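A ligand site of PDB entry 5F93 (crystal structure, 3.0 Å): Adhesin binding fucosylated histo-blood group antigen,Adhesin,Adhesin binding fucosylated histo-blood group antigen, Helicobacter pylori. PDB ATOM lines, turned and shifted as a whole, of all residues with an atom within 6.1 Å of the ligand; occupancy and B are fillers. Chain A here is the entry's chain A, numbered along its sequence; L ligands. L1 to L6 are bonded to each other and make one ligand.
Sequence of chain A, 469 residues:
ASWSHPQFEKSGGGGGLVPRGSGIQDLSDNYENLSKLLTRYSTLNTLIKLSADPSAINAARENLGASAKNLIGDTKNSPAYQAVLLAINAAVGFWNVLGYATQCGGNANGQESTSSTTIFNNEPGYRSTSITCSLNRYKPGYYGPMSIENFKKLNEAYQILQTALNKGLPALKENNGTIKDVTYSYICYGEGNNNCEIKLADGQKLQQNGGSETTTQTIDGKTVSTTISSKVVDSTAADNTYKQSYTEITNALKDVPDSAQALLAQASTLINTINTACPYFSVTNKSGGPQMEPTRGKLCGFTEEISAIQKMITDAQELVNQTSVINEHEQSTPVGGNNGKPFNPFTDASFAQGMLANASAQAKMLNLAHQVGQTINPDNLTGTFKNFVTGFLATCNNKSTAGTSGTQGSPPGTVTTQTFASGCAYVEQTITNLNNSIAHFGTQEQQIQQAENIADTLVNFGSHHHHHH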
ATOM      1  N   CYS A 188     -16.362 -20.302   9.706  1.00  0.00           N
ATOM      2  CA  CYS A 188     -16.244 -20.367   8.219  1.00  0.00           C
ATOM      3  C   CYS A 188     -17.018 -19.278   7.500  1.00  0.00           C
ATOM      4  O   CYS A 188     -18.241 -19.200   7.627  1.00  0.00           O
ATOM      5  CB  CYS A 188     -16.825 -21.655   7.685  1.00  0.00           C
ATOM      6  SG  CYS A 188     -15.865 -23.088   8.100  1.00  0.00           S
ATOM      7  N   TYR A 189     -16.359 -18.485   6.668  1.00  0.00           N
ATOM      8  CA  TYR A 189     -17.129 -17.598   5.815  1.00  0.00           C
ATOM      9  C   TYR A 189     -16.679 -17.513   4.355  1.00  0.00           C
ATOM     10  O   TYR A 189     -15.577 -17.947   4.009  1.00  0.00           O
ATOM     11  CB  TYR A 189     -17.308 -16.228   6.477  1.00  0.00           C
ATOM     12  CG  TYR A 189     -16.128 -15.283   6.595  1.00  0.00           C
ATOM     13  CD1 TYR A 189     -15.664 -14.560   5.494  1.00  0.00           C
ATOM     14  CD2 TYR A 189     -15.553 -15.021   7.833  1.00  0.00           C
ATOM     15  CE1 TYR A 189     -14.625 -13.650   5.623  1.00  0.00           C
ATOM     16  CE2 TYR A 189     -14.516 -14.109   7.976  1.00  0.00           C
ATOM     17  CZ  TYR A 189     -14.055 -13.421   6.863  1.00  0.00           C
ATOM     18  OH  TYR A 189     -13.039 -12.519   7.012  1.00  0.00           O
ATOM     19  N   GLY A 190     -17.584 -17.000   3.518  1.00  0.00           N
ATOM     20  CA  GLY A 190     -17.283 -16.706   2.128  1.00  0.00           C
ATOM     21  C   GLY A 190     -17.969 -17.670   1.203  1.00  0.00           C
ATOM     22  O   GLY A 190     -18.417 -18.724   1.633  1.00  0.00           O
ATOM     23  N   GLU A 191     -18.034 -17.296  -0.071  1.00  0.00           N
ATOM     24  CA  GLU A 191     -18.697 -18.127  -1.075  1.00  0.00           C
ATOM     25  C   GLU A 191     -18.058 -19.505  -1.201  1.00  0.00           C
ATOM     26  O   GLU A 191     -16.826 -19.630  -1.310  1.00  0.00           O
ATOM     27  CB  GLU A 191     -18.682 -17.426  -2.452  1.00  0.00           C
ATOM     28  CG  GLU A 191     -20.021 -16.821  -2.861  1.00  0.00           C
ATOM     29  CD  GLU A 191     -21.148 -17.862  -2.917  1.00  0.00           C
ATOM     30  OE1 GLU A 191     -22.194 -17.671  -2.262  1.00  0.00           O
ATOM     31  OE2 GLU A 191     -20.986 -18.893  -3.606  1.00  0.00           O
ATOM     32  N   GLY A 192     -18.886 -20.539  -1.151  1.00  0.00           N
ATOM     33  CA  GLY A 192     -18.435 -21.910  -1.417  1.00  0.00           C
ATOM     34  C   GLY A 192     -17.533 -22.537  -0.357  1.00  0.00           C
ATOM     35  O   GLY A 192     -17.015 -23.644  -0.579  1.00  0.00           O
ATOM     36  N   ASN A 193     -17.359 -21.848   0.789  1.00  0.00           N
ATOM     37  CA  ASN A 193     -16.575 -22.399   1.910  1.00  0.00           C
ATOM     38  C   ASN A 193     -17.313 -23.537   2.576  1.00  0.00           C
ATOM     39  O   ASN A 193     -18.352 -23.334   3.174  1.00  0.00           O
ATOM     40  CB  ASN A 193     -16.279 -21.334   2.961  1.00  0.00           C
ATOM     41  CG  ASN A 193     -15.342 -21.842   4.044  1.00  0.00           C
ATOM     42  OD1 ASN A 193     -15.102 -23.044   4.173  1.00  0.00           O
ATOM     43  ND2 ASN A 193     -14.777 -20.920   4.818  1.00  0.00           N
ATOM     44  N   ASN A 194     -16.750 -24.725   2.463  1.00  0.00           N
ATOM     45  CA  ASN A 194     -17.390 -25.940   2.937  1.00  0.00           C
ATOM     46  C   ASN A 194     -16.653 -26.592   4.125  1.00  0.00           C
ATOM     47  O   ASN A 194     -16.874 -27.763   4.436  1.00  0.00           O
ATOM     48  CB  ASN A 194     -17.496 -26.945   1.800  1.00  0.00           C
ATOM     49  CG  ASN A 194     -16.142 -27.414   1.295  1.00  0.00           C
ATOM     50  OD1 ASN A 194     -15.118 -26.756   1.456  1.00  0.00           O
ATOM     51  ND2 ASN A 194     -16.136 -28.552   0.641  1.00  0.00           N
ATOM     52  N   GLU A 197     -19.039 -27.822   7.084  1.00  0.00           N
ATOM     53  CA  GLU A 197     -20.004 -28.902   6.897  1.00  0.00           C
ATOM     54  C   GLU A 197     -19.416 -30.108   7.608  1.00  0.00           C
ATOM     55  O   GLU A 197     -18.290 -30.498   7.353  1.00  0.00           O
ATOM     56  CB  GLU A 197     -20.223 -29.176   5.408  1.00  0.00           C
ATOM     57  CG  GLU A 197     -20.886 -28.016   4.651  1.00  0.00           C
ATOM     58  CD  GLU A 197     -20.972 -28.239   3.129  1.00  0.00           C
ATOM     59  OE1 GLU A 197     -21.042 -29.407   2.698  1.00  0.00           O
ATOM     60  OE2 GLU A 197     -20.985 -27.233   2.352  1.00  0.00           O
ATOM     61  N   GLN A 208     -26.710 -27.557  10.260  1.00  0.00           N
ATOM     62  CA  GLN A 208     -25.861 -26.370  10.172  1.00  0.00           C
ATOM     63  C   GLN A 208     -26.245 -25.275  11.163  1.00  0.00           C
ATOM     64  O   GLN A 208     -25.380 -24.603  11.714  1.00  0.00           O
ATOM     65  CB  GLN A 208     -25.850 -25.836   8.736  1.00  0.00           C
ATOM     66  CG  GLN A 208     -24.784 -24.767   8.492  1.00  0.00           C
ATOM     67  CD  GLN A 208     -23.957 -24.993   7.241  1.00  0.00           C
ATOM     68  OE1 GLN A 208     -23.741 -26.142   6.816  1.00  0.00           O
ATOM     69  NE2 GLN A 208     -23.459 -23.897   6.649  1.00  0.00           N
ATOM     70  N   ASN A 209     -27.534 -25.101  11.391  1.00  0.00           N
ATOM     71  CA  ASN A 209     -27.972 -24.100  12.362  1.00  0.00           C
ATOM     72  C   ASN A 209     -28.514 -24.708  13.668  1.00  0.00           C
ATOM     73  O   ASN A 209     -29.579 -25.302  13.691  1.00  0.00           O
ATOM     74  CB  ASN A 209     -29.006 -23.178  11.745  1.00  0.00           C
ATOM     75  CG  ASN A 209     -29.110 -21.876  12.490  1.00  0.00           C
ATOM     76  OD1 ASN A 209     -28.595 -21.749  13.591  1.00  0.00           O
ATOM     77  ND2 ASN A 209     -29.760 -20.899  11.891  1.00  0.00           N
ATOM     78  N   VAL A 232     -25.277 -20.773  12.727  1.00  0.00           N
ATOM     79  CA  VAL A 232     -25.138 -19.788  11.654  1.00  0.00           C
ATOM     80  C   VAL A 232     -25.448 -18.394  12.173  1.00  0.00           C
ATOM     81  O   VAL A 232     -26.397 -18.215  12.924  1.00  0.00           O
ATOM     82  CB  VAL A 232     -26.085 -20.049  10.472  1.00  0.00           C
ATOM     83  CG1 VAL A 232     -25.777 -19.081   9.345  1.00  0.00           C
ATOM     84  CG2 VAL A 232     -25.981 -21.496  10.002  1.00  0.00           C
ATOM     85  N   VAL A 233     -24.665 -17.421  11.731  1.00  0.00           N
ATOM     86  CA  VAL A 233     -24.755 -16.024  12.165  1.00  0.00           C
ATOM     87  C   VAL A 233     -24.822 -15.203  10.877  1.00  0.00           C
ATOM     88  O   VAL A 233     -23.922 -15.271  10.049  1.00  0.00           O
ATOM     89  CB  VAL A 233     -23.500 -15.590  12.999  1.00  0.00           C
ATOM     90  CG1 VAL A 233     -23.515 -14.098  13.325  1.00  0.00           C
ATOM     91  CG2 VAL A 233     -23.385 -16.387  14.296  1.00  0.00           C
ATOM     92  N   ASP A 234     -25.895 -14.440  10.696  1.00  0.00           N
ATOM     93  CA  ASP A 234     -26.098 -13.668   9.471  1.00  0.00           C
ATOM     94  C   ASP A 234     -25.326 -12.347   9.514  1.00  0.00           C
ATOM     95  O   ASP A 234     -24.899 -11.904  10.575  1.00  0.00           O
ATOM     96  CB  ASP A 234     -27.591 -13.411   9.252  1.00  0.00           C
ATOM     97  CG  ASP A 234     -27.916 -12.975   7.835  1.00  0.00           C
ATOM     98  OD1 ASP A 234     -27.816 -13.817   6.911  1.00  0.00           O
ATOM     99  OD2 ASP A 234     -28.266 -11.787   7.639  1.00  0.00           O
ATOM    100  N   SER A 235     -25.159 -11.757   8.338  1.00  0.00           N
ATOM    101  CA  SER A 235     -24.343 -10.558   8.103  1.00  0.00           C
ATOM    102  C   SER A 235     -24.846  -9.278   8.770  1.00  0.00           C
ATOM    103  O   SER A 235     -24.058  -8.382   9.111  1.00  0.00           O
ATOM    104  CB  SER A 235     -24.286 -10.301   6.600  1.00  0.00           C
ATOM    105  OG  SER A 235     -25.551 -10.597   6.011  1.00  0.00           O
ATOM    106  N   LYS A 243     -19.012  -8.440   9.139  1.00  0.00           N
ATOM    107  CA  LYS A 243     -20.089  -8.028   8.214  1.00  0.00           C
ATOM    108  C   LYS A 243     -20.271  -9.004   7.039  1.00  0.00           C
ATOM    109  O   LYS A 243     -20.452  -8.603   5.880  1.00  0.00           O
ATOM    110  CB  LYS A 243     -19.905  -6.565   7.757  1.00  0.00           C
ATOM    111  CG  LYS A 243     -20.255  -5.559   8.872  1.00  0.00           C
ATOM    112  CD  LYS A 243     -20.228  -4.098   8.449  1.00  0.00           C
ATOM    113  CE  LYS A 243     -20.579  -3.216   9.638  1.00  0.00           C
ATOM    114  NZ  LYS A 243     -20.376  -1.772   9.369  1.00  0.00           N
ATOM    115  N   GLN A 244     -20.240 -10.296   7.376  1.00  0.00           N
ATOM    116  CA  GLN A 244     -20.438 -11.383   6.429  1.00  0.00           C
ATOM    117  C   GLN A 244     -20.980 -12.594   7.154  1.00  0.00           C
ATOM    118  O   GLN A 244     -20.527 -12.867   8.265  1.00  0.00           O
ATOM    119  CB  GLN A 244     -19.113 -11.757   5.793  1.00  0.00           C
ATOM    120  CG  GLN A 244     -18.794 -10.998   4.532  1.00  0.00           C
ATOM    121  CD  GLN A 244     -17.855 -11.774   3.641  1.00  0.00           C
ATOM    122  OE1 GLN A 244     -18.218 -12.820   3.095  1.00  0.00           O
ATOM    123  NE2 GLN A 244     -16.626 -11.298   3.536  1.00  0.00           N
ATOM    124  N   SER A 245     -21.918 -13.314   6.543  1.00  0.00           N
ATOM    125  CA  SER A 245     -22.643 -14.389   7.233  1.00  0.00           C
ATOM    126  C   SER A 245     -21.712 -15.577   7.433  1.00  0.00           C
ATOM    127  O   SER A 245     -21.063 -16.007   6.481  1.00  0.00           O
ATOM    128  CB  SER A 245     -23.885 -14.846   6.437  1.00  0.00           C
ATOM    129  OG  SER A 245     -24.858 -13.821   6.266  1.00  0.00           O
ATOM    130  N   TYR A 246     -21.642 -16.105   8.663  1.00  0.00           N
ATOM    131  CA  TYR A 246     -20.696 -17.183   8.963  1.00  0.00           C
ATOM    132  C   TYR A 246     -21.280 -18.376   9.711  1.00  0.00           C
ATOM    133  O   TYR A 246     -22.394 -18.321  10.207  1.00  0.00           O
ATOM    134  CB  TYR A 246     -19.477 -16.668   9.709  1.00  0.00           C
ATOM    135  CG  TYR A 246     -19.726 -16.134  11.098  1.00  0.00           C
ATOM    136  CD1 TYR A 246     -19.894 -16.980  12.201  1.00  0.00           C
ATOM    137  CD2 TYR A 246     -19.706 -14.758  11.329  1.00  0.00           C
ATOM    138  CE1 TYR A 246     -20.076 -16.467  13.484  1.00  0.00           C
ATOM    139  CE2 TYR A 246     -19.895 -14.239  12.597  1.00  0.00           C
ATOM    140  CZ  TYR A 246     -20.083 -15.086  13.655  1.00  0.00           C
ATOM    141  OH  TYR A 246     -20.262 -14.519  14.877  1.00  0.00           O
ATOM    142  N   THR A 247     -20.505 -19.440   9.731  1.00  0.00           N
ATOM    143  CA  THR A 247     -20.830 -20.636  10.447  1.00  0.00           C
ATOM    144  C   THR A 247     -19.759 -20.864  11.506  1.00  0.00           C
ATOM    145  O   THR A 247     -18.570 -20.892  11.201  1.00  0.00           O
ATOM    146  CB  THR A 247     -20.816 -21.846   9.522  1.00  0.00           C
ATOM    147  OG1 THR A 247     -21.533 -21.554   8.306  1.00  0.00           O
ATOM    148  CG2 THR A 247     -21.425 -23.072  10.242  1.00  0.00           C
HETATM  149  C1  LIG L   1     -23.346 -10.356  -4.412  1.00  0.00           C
HETATM  150  C2  LIG L   1     -22.314  -9.988  -3.323  1.00  0.00           C
HETATM  151  C3  LIG L   1     -22.119 -11.168  -2.381  1.00  0.00           C
HETATM  152  C4  LIG L   1     -23.443 -11.393  -1.649  1.00  0.00           C
HETATM  153  C5  LIG L   1     -24.560 -11.637  -2.691  1.00  0.00           C
HETATM  154  C6  LIG L   1     -25.970 -11.604  -2.080  1.00  0.00           C
HETATM  155  O1  LIG L   1     -22.967 -11.466  -5.203  1.00  0.00           O
HETATM  156  O2  LIG L   1     -21.088  -9.534  -3.861  1.00  0.00           O
HETATM  157  O3  LIG L   1     -21.074 -10.907  -1.468  1.00  0.00           O
HETATM  158  O4  LIG L   1     -23.264 -12.436  -0.683  1.00  0.00           O
HETATM  159  O5  LIG L   1     -24.565 -10.693  -3.775  1.00  0.00           O
HETATM  160  O6  LIG L   1     -26.960 -11.772  -3.073  1.00  0.00           O
HETATM  161  C1  LG2 L   2     -24.019 -12.207   0.553  1.00  0.00           C
HETATM  162  C2  LG2 L   2     -23.983 -13.453   1.442  1.00  0.00           C
HETATM  163  C3  LG2 L   2     -24.980 -13.272   2.573  1.00  0.00           C
HETATM  164  C4  LG2 L   2     -24.613 -11.993   3.293  1.00  0.00           C
HETATM  165  C5  LG2 L   2     -24.557 -10.791   2.345  1.00  0.00           C
HETATM  166  C6  LG2 L   2     -24.242  -9.476   3.079  1.00  0.00           C
HETATM  167  O1  LG2 L   2     -24.347 -14.620   0.741  1.00  0.00           O
HETATM  168  O2  LG2 L   2     -24.881 -14.374   3.450  1.00  0.00           O
HETATM  169  O3  LG2 L   2     -23.325 -12.192   3.837  1.00  0.00           O
HETATM  170  O4  LG2 L   2     -23.623 -11.068   1.315  1.00  0.00           O
HETATM  171  O5  LG2 L   2     -23.208  -8.753   2.460  1.00  0.00           O
HETATM  172  C1  LG3 L   3     -25.851 -15.430   3.260  1.00  0.00           C
HETATM  173  C2  LG3 L   3     -25.108 -16.752   3.297  1.00  0.00           C
HETATM  174  C3  LG3 L   3     -26.065 -17.916   3.259  1.00  0.00           C
HETATM  175  C4  LG3 L   3     -27.043 -17.800   4.418  1.00  0.00           C
HETATM  176  C5  LG3 L   3     -27.758 -16.456   4.248  1.00  0.00           C
HETATM  177  C6  LG3 L   3     -28.853 -16.206   5.278  1.00  0.00           C
HETATM  178  C7  LG3 L   3     -22.867 -17.080   2.281  1.00  0.00           C
HETATM  179  C8  LG3 L   3     -22.163 -17.347   0.979  1.00  0.00           C
HETATM  180  N1  LG3 L   3     -24.201 -16.985   2.190  1.00  0.00           N
HETATM  181  O1  LG3 L   3     -25.254 -19.080   3.340  1.00  0.00           O
HETATM  182  O2  LG3 L   3     -27.979 -18.860   4.325  1.00  0.00           O
HETATM  183  O3  LG3 L   3     -26.802 -15.424   4.309  1.00  0.00           O
HETATM  184  O4  LG3 L   3     -28.310 -16.285   6.575  1.00  0.00           O
HETATM  185  O5  LG3 L   3     -22.169 -16.963   3.286  1.00  0.00           O
HETATM  186  C1  LG4 L   4     -25.369 -20.011   2.246  1.00  0.00           C
HETATM  187  C2  LG4 L   4     -24.544 -21.266   2.563  1.00  0.00           C
HETATM  188  C3  LG4 L   4     -24.722 -22.341   1.481  1.00  0.00           C
HETATM  189  C4  LG4 L   4     -26.217 -22.603   1.153  1.00  0.00           C
HETATM  190  C5  LG4 L   4     -26.914 -21.246   0.947  1.00  0.00           C
HETATM  191  C6  LG4 L   4     -28.411 -21.365   0.757  1.00  0.00           C
HETATM  192  O1  LG4 L   4     -23.167 -20.935   2.747  1.00  0.00           O
HETATM  193  O2  LG4 L   4     -23.998 -23.514   1.789  1.00  0.00           O
HETATM  194  O3  LG4 L   4     -26.912 -23.403   2.095  1.00  0.00           O
HETATM  195  O4  LG4 L   4     -26.711 -20.384   2.033  1.00  0.00           O
HETATM  196  O5  LG4 L   4     -28.573 -21.512  -0.629  1.00  0.00           O
HETATM  197  C1  LG5 L   5     -28.300 -19.503   5.576  1.00  0.00           C
HETATM  198  C2  LG5 L   5     -29.733 -19.994   5.442  1.00  0.00           C
HETATM  199  C3  LG5 L   5     -29.843 -21.130   4.428  1.00  0.00           C
HETATM  200  C4  LG5 L   5     -28.883 -22.259   4.777  1.00  0.00           C
HETATM  201  C5  LG5 L   5     -27.483 -21.731   5.069  1.00  0.00           C
HETATM  202  C6  LG5 L   5     -26.602 -22.848   5.637  1.00  0.00           C
HETATM  203  O1  LG5 L   5     -30.528 -18.908   5.005  1.00  0.00           O
HETATM  204  O2  LG5 L   5     -31.160 -21.631   4.434  1.00  0.00           O
HETATM  205  O3  LG5 L   5     -29.372 -22.979   5.889  1.00  0.00           O
HETATM  206  O4  LG5 L   5     -27.469 -20.593   5.937  1.00  0.00           O
HETATM  207  C1  LG6 L   6     -22.558 -21.519   3.925  1.00  0.00           C
HETATM  208  C2  LG6 L   6     -21.035 -21.306   3.811  1.00  0.00           C
HETATM  209  C3  LG6 L   6     -20.628 -19.840   3.987  1.00  0.00           C
HETATM  210  C4  LG6 L   6     -21.251 -19.246   5.257  1.00  0.00           C
HETATM  211  C5  LG6 L   6     -22.735 -19.636   5.409  1.00  0.00           C
HETATM  212  C6  LG6 L   6     -23.278 -19.209   6.771  1.00  0.00           C
HETATM  213  O1  LG6 L   6     -20.544 -21.840   2.595  1.00  0.00           O
HETATM  214  O2  LG6 L   6     -19.213 -19.712   4.062  1.00  0.00           O
HETATM  215  O3  LG6 L   6     -20.508 -19.579   6.422  1.00  0.00           O
HETATM  216  O4  LG6 L   6     -23.020 -21.021   5.182  1.00  0.00           O
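N of Gly 190 sits at hydrogen-bond distance from O2 of LG6 L6 (3.2 Å).
An oxygen (O4) of LG6 L6 lies within hydrogen-bond range of the side-chain amide nitrogen (NE2) of Gln 208, 3.3 Å away.
The side-chain hydroxyl (OG) of Ser 245 sits at hydrogen-bond distance from an oxygen (O2) of LG2 L2 (2.9 Å).
The backbone NH (N) of Ser 245 is in hydrogen-bond range of an oxygen (O3) of LG2 L2 (3.2 Å).
The side-chain hydroxyl (OG) of Ser 235 sits close to an oxygen (O3) of LG2 L2 (3.5 Å).
The backbone carbonyl oxygen (O) of Asn 193 is in hydrogen-bond range of an oxygen (O1) of LG6 L6 (2.7 Å).
O3 of LG6 L6 is in hydrogen-bond range of OG1 of Thr 247, at 2.9 Å.
The side-chain carboxylate (OD1) of Asp 234 sits at hydrogen-bond distance from an oxygen (O4) of LG3 L3.
N of Thr 247 lies within hydrogen-bond range of O3 of LG6 L6 (3.3 Å).
O of Gly 190 is in hydrogen-bond range of O2 of LG6 L6, 2.7 Å away.
O3 of LG6 L6 is in hydrogen-bond range of O of Cys 188.
The backbone NH (N) of Tyr 246 is in hydrogen-bond range of the backbone carbonyl oxygen (O) of Val 233 (2.8 Å).
The side-chain hydroxyl (OG) of Ser 245 is in hydrogen-bond range of the side-chain carboxylate (OD1) of Asp 234, at 3.0 Å.
OD2 of Asp 234 lies within hydrogen-bond range of OG of Ser 235 (3.4 Å).
The backbone NH (N) of Cys 188 sits at hydrogen-bond distance from the backbone carbonyl oxygen (O) of Thr 247 (2.7 Å).
The side-chain hydroxyl of Thr 247 is in hydrogen-bond range of the side-chain amide nitrogen of Gln 208 (3.5 Å).
OG of Ser 245 lies within hydrogen-bond range of N of Ser 235 (2.9 Å).
ND2 of Asn 193 lies within hydrogen-bond range of O of Tyr 189.
Residues that only touch the ligand: Tyr 189 (3.4 Å), Glu 191 (3.3 Å), Val 232 (3.6 Å), Gln 244 (3.96 Å) and Tyr 246 (3.5 Å).
Hydrophobic or aromatic side chains within 4 Å of the ligand: Val 232.
Of the 19 residues printed, 13 come within 4 Å of the ligand.
The nearest printed residue that does not touch the ligand is Gly 192 (4.3 Å).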
